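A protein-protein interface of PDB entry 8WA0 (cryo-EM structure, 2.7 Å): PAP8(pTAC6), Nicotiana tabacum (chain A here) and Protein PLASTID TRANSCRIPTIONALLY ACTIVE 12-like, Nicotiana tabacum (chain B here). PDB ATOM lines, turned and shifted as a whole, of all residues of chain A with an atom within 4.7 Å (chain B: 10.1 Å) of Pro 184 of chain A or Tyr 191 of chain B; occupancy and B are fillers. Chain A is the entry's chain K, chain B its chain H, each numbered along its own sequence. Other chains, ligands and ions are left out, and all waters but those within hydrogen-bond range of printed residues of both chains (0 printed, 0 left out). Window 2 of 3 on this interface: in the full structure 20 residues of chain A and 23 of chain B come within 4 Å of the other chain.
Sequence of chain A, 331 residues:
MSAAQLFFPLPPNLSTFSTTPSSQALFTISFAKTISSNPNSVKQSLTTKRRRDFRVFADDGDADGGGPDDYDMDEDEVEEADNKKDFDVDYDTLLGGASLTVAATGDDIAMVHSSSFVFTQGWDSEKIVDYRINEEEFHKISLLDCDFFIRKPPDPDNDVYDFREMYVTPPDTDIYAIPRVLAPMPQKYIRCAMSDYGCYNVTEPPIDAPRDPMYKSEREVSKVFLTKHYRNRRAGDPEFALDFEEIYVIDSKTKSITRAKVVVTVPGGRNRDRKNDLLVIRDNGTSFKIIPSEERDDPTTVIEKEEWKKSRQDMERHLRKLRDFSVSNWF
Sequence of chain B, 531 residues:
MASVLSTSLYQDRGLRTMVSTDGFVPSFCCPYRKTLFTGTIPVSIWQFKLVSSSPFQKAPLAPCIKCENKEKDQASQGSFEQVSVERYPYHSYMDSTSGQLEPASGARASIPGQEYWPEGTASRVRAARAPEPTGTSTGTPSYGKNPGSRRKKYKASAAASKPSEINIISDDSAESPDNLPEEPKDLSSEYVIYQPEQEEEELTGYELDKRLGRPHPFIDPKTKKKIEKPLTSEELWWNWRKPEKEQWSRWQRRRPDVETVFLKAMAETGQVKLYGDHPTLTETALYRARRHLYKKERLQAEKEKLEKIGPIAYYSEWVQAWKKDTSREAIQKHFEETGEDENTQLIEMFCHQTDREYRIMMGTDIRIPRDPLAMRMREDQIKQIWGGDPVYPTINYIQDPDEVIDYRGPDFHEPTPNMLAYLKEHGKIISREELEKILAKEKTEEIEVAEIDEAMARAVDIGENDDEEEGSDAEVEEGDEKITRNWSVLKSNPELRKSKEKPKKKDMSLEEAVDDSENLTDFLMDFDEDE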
ATOM      1  N   ALA A 183       0.654  15.262 -16.115  1.00  0.00           N
ATOM      2  CA  ALA A 183       1.698  14.429 -15.531  1.00  0.00           C
ATOM      3  C   ALA A 183       1.172  13.076 -15.108  1.00  0.00           C
ATOM      4  O   ALA A 183      -0.030  12.860 -15.090  1.00  0.00           O
ATOM      5  CB  ALA A 183       2.312  15.140 -14.346  1.00  0.00           C
ATOM      6  N   PRO A 184       2.070  12.143 -14.774  1.00  0.00           N
ATOM      7  CA  PRO A 184       1.564  10.874 -14.262  1.00  0.00           C
ATOM      8  C   PRO A 184       0.818  11.092 -12.974  1.00  0.00           C
ATOM      9  O   PRO A 184       1.273  11.858 -12.137  1.00  0.00           O
ATOM     10  CB  PRO A 184       2.840  10.079 -13.973  1.00  0.00           C
ATOM     11  CG  PRO A 184       3.990  11.004 -14.211  1.00  0.00           C
ATOM     12  CD  PRO A 184       3.486  12.044 -15.155  1.00  0.00           C
ATOM     13  N   MET A 185      -0.303  10.410 -12.782  1.00  0.00           N
ATOM     14  CA  MET A 185      -1.074  10.550 -11.555  1.00  0.00           C
ATOM     15  C   MET A 185      -1.077   9.275 -10.734  1.00  0.00           C
ATOM     16  O   MET A 185      -0.933   8.191 -11.280  1.00  0.00           O
ATOM     17  CB  MET A 185      -2.494  10.989 -11.879  1.00  0.00           C
ATOM     18  CG  MET A 185      -2.602  12.463 -12.226  1.00  0.00           C
ATOM     19  SD  MET A 185      -1.963  13.538 -10.927  1.00  0.00           S
ATOM     20  CE  MET A 185      -1.242  14.860 -11.893  1.00  0.00           C
ATOM     21  N   PRO A 186      -1.228   9.395  -9.413  1.00  0.00           N
ATOM     22  CA  PRO A 186      -1.162   8.202  -8.567  1.00  0.00           C
ATOM     23  C   PRO A 186      -2.297   7.239  -8.846  1.00  0.00           C
ATOM     24  O   PRO A 186      -3.407   7.676  -9.120  1.00  0.00           O
ATOM     25  CB  PRO A 186      -1.322   8.751  -7.158  1.00  0.00           C
ATOM     26  CG  PRO A 186      -1.064  10.203  -7.249  1.00  0.00           C
ATOM     27  CD  PRO A 186      -1.401  10.629  -8.634  1.00  0.00           C
ATOM     28  N   TYR A 248       1.629  17.920  -5.638  1.00  0.00           N
ATOM     29  CA  TYR A 248       0.901  18.039  -6.867  1.00  0.00           C
ATOM     30  C   TYR A 248       0.236  19.381  -6.934  1.00  0.00           C
ATOM     31  O   TYR A 248      -0.237  19.854  -5.918  1.00  0.00           O
ATOM     32  CB  TYR A 248      -0.160  16.988  -6.885  1.00  0.00           C
ATOM     33  CG  TYR A 248       0.336  15.584  -6.920  1.00  0.00           C
ATOM     34  CD1 TYR A 248       0.892  15.067  -8.066  1.00  0.00           C
ATOM     35  CD2 TYR A 248       0.227  14.767  -5.817  1.00  0.00           C
ATOM     36  CE1 TYR A 248       1.350  13.776  -8.107  1.00  0.00           C
ATOM     37  CE2 TYR A 248       0.680  13.474  -5.850  1.00  0.00           C
ATOM     38  CZ  TYR A 248       1.248  12.989  -6.999  1.00  0.00           C
ATOM     39  OH  TYR A 248       1.707  11.697  -7.049  1.00  0.00           O
ATOM     40  N   ARG A 259       2.579  17.647 -11.573  1.00  0.00           N
ATOM     41  CA  ARG A 259       3.403  17.312 -10.435  1.00  0.00           C
ATOM     42  C   ARG A 259       4.599  18.185 -10.418  1.00  0.00           C
ATOM     43  O   ARG A 259       5.136  18.524 -11.458  1.00  0.00           O
ATOM     44  CB  ARG A 259       3.850  15.868 -10.479  1.00  0.00           C
ATOM     45  CG  ARG A 259       4.520  15.327  -9.229  1.00  0.00           C
ATOM     46  CD  ARG A 259       5.281  14.069  -9.588  1.00  0.00           C
ATOM     47  NE  ARG A 259       5.320  13.069  -8.532  1.00  0.00           N
ATOM     48  CZ  ARG A 259       6.303  12.945  -7.652  1.00  0.00           C
ATOM     49  NH1 ARG A 259       7.334  13.773  -7.680  1.00  0.00           N
ATOM     50  NH2 ARG A 259       6.252  11.994  -6.735  1.00  0.00           N
ATOM     51  N   ALA A 260       5.012  18.592  -9.242  1.00  0.00           N
ATOM     52  CA  ALA A 260       6.133  19.478  -9.107  1.00  0.00           C
ATOM     53  C   ALA A 260       7.510  18.886  -9.277  1.00  0.00           C
ATOM     54  O   ALA A 260       7.689  17.685  -9.101  1.00  0.00           O
ATOM     55  CB  ALA A 260       6.049  20.130  -7.752  1.00  0.00           C
ATOM     56  N   LYS A 261       8.497  19.708  -9.604  1.00  0.00           N
ATOM     57  CA  LYS A 261       9.860  19.234  -9.662  1.00  0.00           C
ATOM     58  C   LYS A 261      10.620  19.802  -8.498  1.00  0.00           C
ATOM     59  O   LYS A 261      10.815  20.998  -8.423  1.00  0.00           O
ATOM     60  CB  LYS A 261      10.494  19.688 -10.947  1.00  0.00           C
ATOM     61  CG  LYS A 261       9.671  19.369 -12.180  1.00  0.00           C
ATOM     62  CD  LYS A 261      10.273  20.011 -13.415  1.00  0.00           C
ATOM     63  CE  LYS A 261       9.373  19.820 -14.624  1.00  0.00           C
ATOM     64  NZ  LYS A 261       9.930  20.488 -15.833  1.00  0.00           N
ATOM     65  N   VAL A 262      11.002  18.960  -7.553  1.00  0.00           N
ATOM     66  CA  VAL A 262      11.691  19.428  -6.367  1.00  0.00           C
ATOM     67  C   VAL A 262      13.178  19.192  -6.477  1.00  0.00           C
ATOM     68  O   VAL A 262      13.598  18.202  -7.053  1.00  0.00           O
ATOM     69  CB  VAL A 262      11.193  18.693  -5.129  1.00  0.00           C
ATOM     70  N   LEU B 187      15.784   4.933 -10.962  1.00  0.00           N
ATOM     71  CA  LEU B 187      14.940   4.988  -9.775  1.00  0.00           C
ATOM     72  C   LEU B 187      14.217   6.323  -9.687  1.00  0.00           C
ATOM     73  O   LEU B 187      12.995   6.384  -9.820  1.00  0.00           O
ATOM     74  CB  LEU B 187      15.777   4.761  -8.514  1.00  0.00           C
ATOM     75  CG  LEU B 187      15.025   4.688  -7.182  1.00  0.00           C
ATOM     76  CD1 LEU B 187      14.043   3.526  -7.181  1.00  0.00           C
ATOM     77  CD2 LEU B 187      16.004   4.566  -6.024  1.00  0.00           C
ATOM     78  N   SER B 188      14.969   7.396  -9.465  1.00  0.00           N
ATOM     79  CA  SER B 188      14.364   8.717  -9.355  1.00  0.00           C
ATOM     80  C   SER B 188      13.734   9.157 -10.664  1.00  0.00           C
ATOM     81  O   SER B 188      14.268   8.892 -11.737  1.00  0.00           O
ATOM     82  CB  SER B 188      15.399   9.749  -8.897  1.00  0.00           C
ATOM     83  OG  SER B 188      16.452   9.866  -9.838  1.00  0.00           O
ATOM     84  N   SER B 189      12.594   9.818 -10.578  1.00  0.00           N
ATOM     85  CA  SER B 189      11.937  10.312 -11.774  1.00  0.00           C
ATOM     86  C   SER B 189      12.535  11.624 -12.153  1.00  0.00           C
ATOM     87  O   SER B 189      13.396  12.140 -11.446  1.00  0.00           O
ATOM     88  CB  SER B 189      10.447  10.474 -11.535  1.00  0.00           C
ATOM     89  OG  SER B 189       9.846   9.235 -11.210  1.00  0.00           O
ATOM     90  N   GLU B 190      12.096  12.196 -13.257  1.00  0.00           N
ATOM     91  CA  GLU B 190      12.553  13.524 -13.617  1.00  0.00           C
ATOM     92  C   GLU B 190      12.079  14.424 -12.520  1.00  0.00           C
ATOM     93  O   GLU B 190      12.660  15.473 -12.271  1.00  0.00           O
ATOM     94  CB  GLU B 190      11.923  13.949 -14.927  1.00  0.00           C
ATOM     95  CG  GLU B 190      12.527  15.196 -15.556  1.00  0.00           C
ATOM     96  CD  GLU B 190      11.740  16.456 -15.248  1.00  0.00           C
ATOM     97  OE1 GLU B 190      10.571  16.342 -14.825  1.00  0.00           O
ATOM     98  OE2 GLU B 190      12.289  17.562 -15.434  1.00  0.00           O
ATOM     99  N   TYR B 191      11.027  14.018 -11.844  1.00  0.00           N
ATOM    100  CA  TYR B 191      10.435  14.816 -10.808  1.00  0.00           C
ATOM    101  C   TYR B 191      11.256  15.161  -9.607  1.00  0.00           C
ATOM    102  O   TYR B 191      11.138  16.276  -9.114  1.00  0.00           O
ATOM    103  CB  TYR B 191       9.073  14.253 -10.533  1.00  0.00           C
ATOM    104  CG  TYR B 191       8.256  14.367 -11.781  1.00  0.00           C
ATOM    105  CD1 TYR B 191       8.177  15.573 -12.448  1.00  0.00           C
ATOM    106  CD2 TYR B 191       7.611  13.277 -12.324  1.00  0.00           C
ATOM    107  CE1 TYR B 191       7.457  15.701 -13.608  1.00  0.00           C
ATOM    108  CE2 TYR B 191       6.886  13.397 -13.488  1.00  0.00           C
ATOM    109  CZ  TYR B 191       6.814  14.615 -14.121  1.00  0.00           C
ATOM    110  OH  TYR B 191       6.099  14.758 -15.280  1.00  0.00           O
ATOM    111  N   VAL B 192      12.087  14.281  -9.103  1.00  0.00           N
ATOM    112  CA  VAL B 192      12.985  14.686  -8.045  1.00  0.00           C
ATOM    113  C   VAL B 192      14.446  14.694  -8.450  1.00  0.00           C
ATOM    114  O   VAL B 192      14.942  13.685  -8.940  1.00  0.00           O
ATOM    115  CB  VAL B 192      12.895  13.801  -6.862  1.00  0.00           C
ATOM    116  CG1 VAL B 192      13.761  14.412  -5.781  1.00  0.00           C
ATOM    117  CG2 VAL B 192      11.437  13.647  -6.484  1.00  0.00           C
ATOM    118  N   ILE B 193      15.153  15.807  -8.258  1.00  0.00           N
ATOM    119  CA  ILE B 193      16.567  15.920  -8.631  1.00  0.00           C
ATOM    120  C   ILE B 193      17.472  16.225  -7.427  1.00  0.00           C
ATOM    121  O   ILE B 193      17.181  17.143  -6.670  1.00  0.00           O
ATOM    122  CB  ILE B 193      16.742  17.004  -9.701  1.00  0.00           C
ATOM    123  CG1 ILE B 193      15.856  16.729 -10.912  1.00  0.00           C
ATOM    124  CG2 ILE B 193      18.197  17.119 -10.122  1.00  0.00           C
ATOM    125  CD1 ILE B 193      16.281  15.522 -11.720  1.00  0.00           C
ATOM    126  N   TYR B 194      18.555  15.477  -7.231  1.00  0.00           N
ATOM    127  CA  TYR B 194      19.447  15.703  -6.091  1.00  0.00           C
ATOM    128  C   TYR B 194      20.704  16.490  -6.420  1.00  0.00           C
ATOM    129  O   TYR B 194      21.466  16.089  -7.287  1.00  0.00           O
ATOM    130  CB  TYR B 194      19.828  14.405  -5.426  1.00  0.00           C
ATOM    131  CG  TYR B 194      18.765  13.833  -4.549  1.00  0.00           C
ATOM    132  CD1 TYR B 194      18.693  14.178  -3.212  1.00  0.00           C
ATOM    133  CD2 TYR B 194      17.827  12.954  -5.051  1.00  0.00           C
ATOM    134  CE1 TYR B 194      17.713  13.661  -2.396  1.00  0.00           C
ATOM    135  CE2 TYR B 194      16.841  12.435  -4.246  1.00  0.00           C
ATOM    136  CZ  TYR B 194      16.791  12.790  -2.920  1.00  0.00           C
ATOM    137  OH  TYR B 194      15.810  12.281  -2.105  1.00  0.00           O
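Hydrophobic or aromatic side chains of chain B within 4 Å of the printed part of chain A: Tyr 191. Along chain B the printed residues that touch a printed residue of chain A span positions 190 to 193. Of the 9 printed residues of chain A, 6 touch a printed residue of chain B. Along chain A the printed residues that touch a printed residue of chain B span positions 183 to 262.
Pro 184 of chain A touches just one residue of chain B: Tyr 191 (3.8 Å). No residue of chain B comes within 4 Å of Met 185 of chain A. Tyr 248 of chain A touches none of the printed residues of chain B. Of chain B, only Tyr 191 (3.4 Å) comes within 4 Å of Arg 259 of chain A. Of the printed residues of chain B, Ala 260 of chain A touches Tyr 191 (3.7 Å). Of the printed residues of chain A, Glu 190 of chain B touches Lys 261 (3.7 Å). Tyr 191 of chain B touches just these residues of chain A: Ala 183, Pro 184, Arg 259, Ala 260, Lys 261 and Val 262. Of the printed residues of chain A, Val 192 of chain B touches Val 262. Of the printed residues of chain A, Ile 193 of chain B touches Val 262. The nearest printed residue of chain A that does not touch Tyr 191 of chain B is Tyr 248 of chain A (7.6 Å).
CB of Ala 183 of chain A touches OH of Tyr 191 of chain B, 3.9 Å away. Pro 184 of chain A touches Tyr 191 of chain B. NH1 of Arg 259 of chain A touches CB of Tyr 191 of chain B, 3.4 Å away. Ala 260 of chain A touches Tyr 191 of chain B. Lys 261 of chain A touches Tyr 191 of chain B. CA of Val 192 of chain B touches O of Val 262 of chain A, at 3.7 Å.
OE2 of Glu 190 of chain B is in salt-bridge range of NZ of Lys 261 of chain A (3.8 Å). The backbone NH (N) of Val 262 of chain A lies within hydrogen-bond range of the backbone carbonyl oxygen (O) of Tyr 191 of chain B (3.1 Å). O of Val 262 of chain A lies within hydrogen-bond range of N of Ile 193 of chain B, 3.1 Å away.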
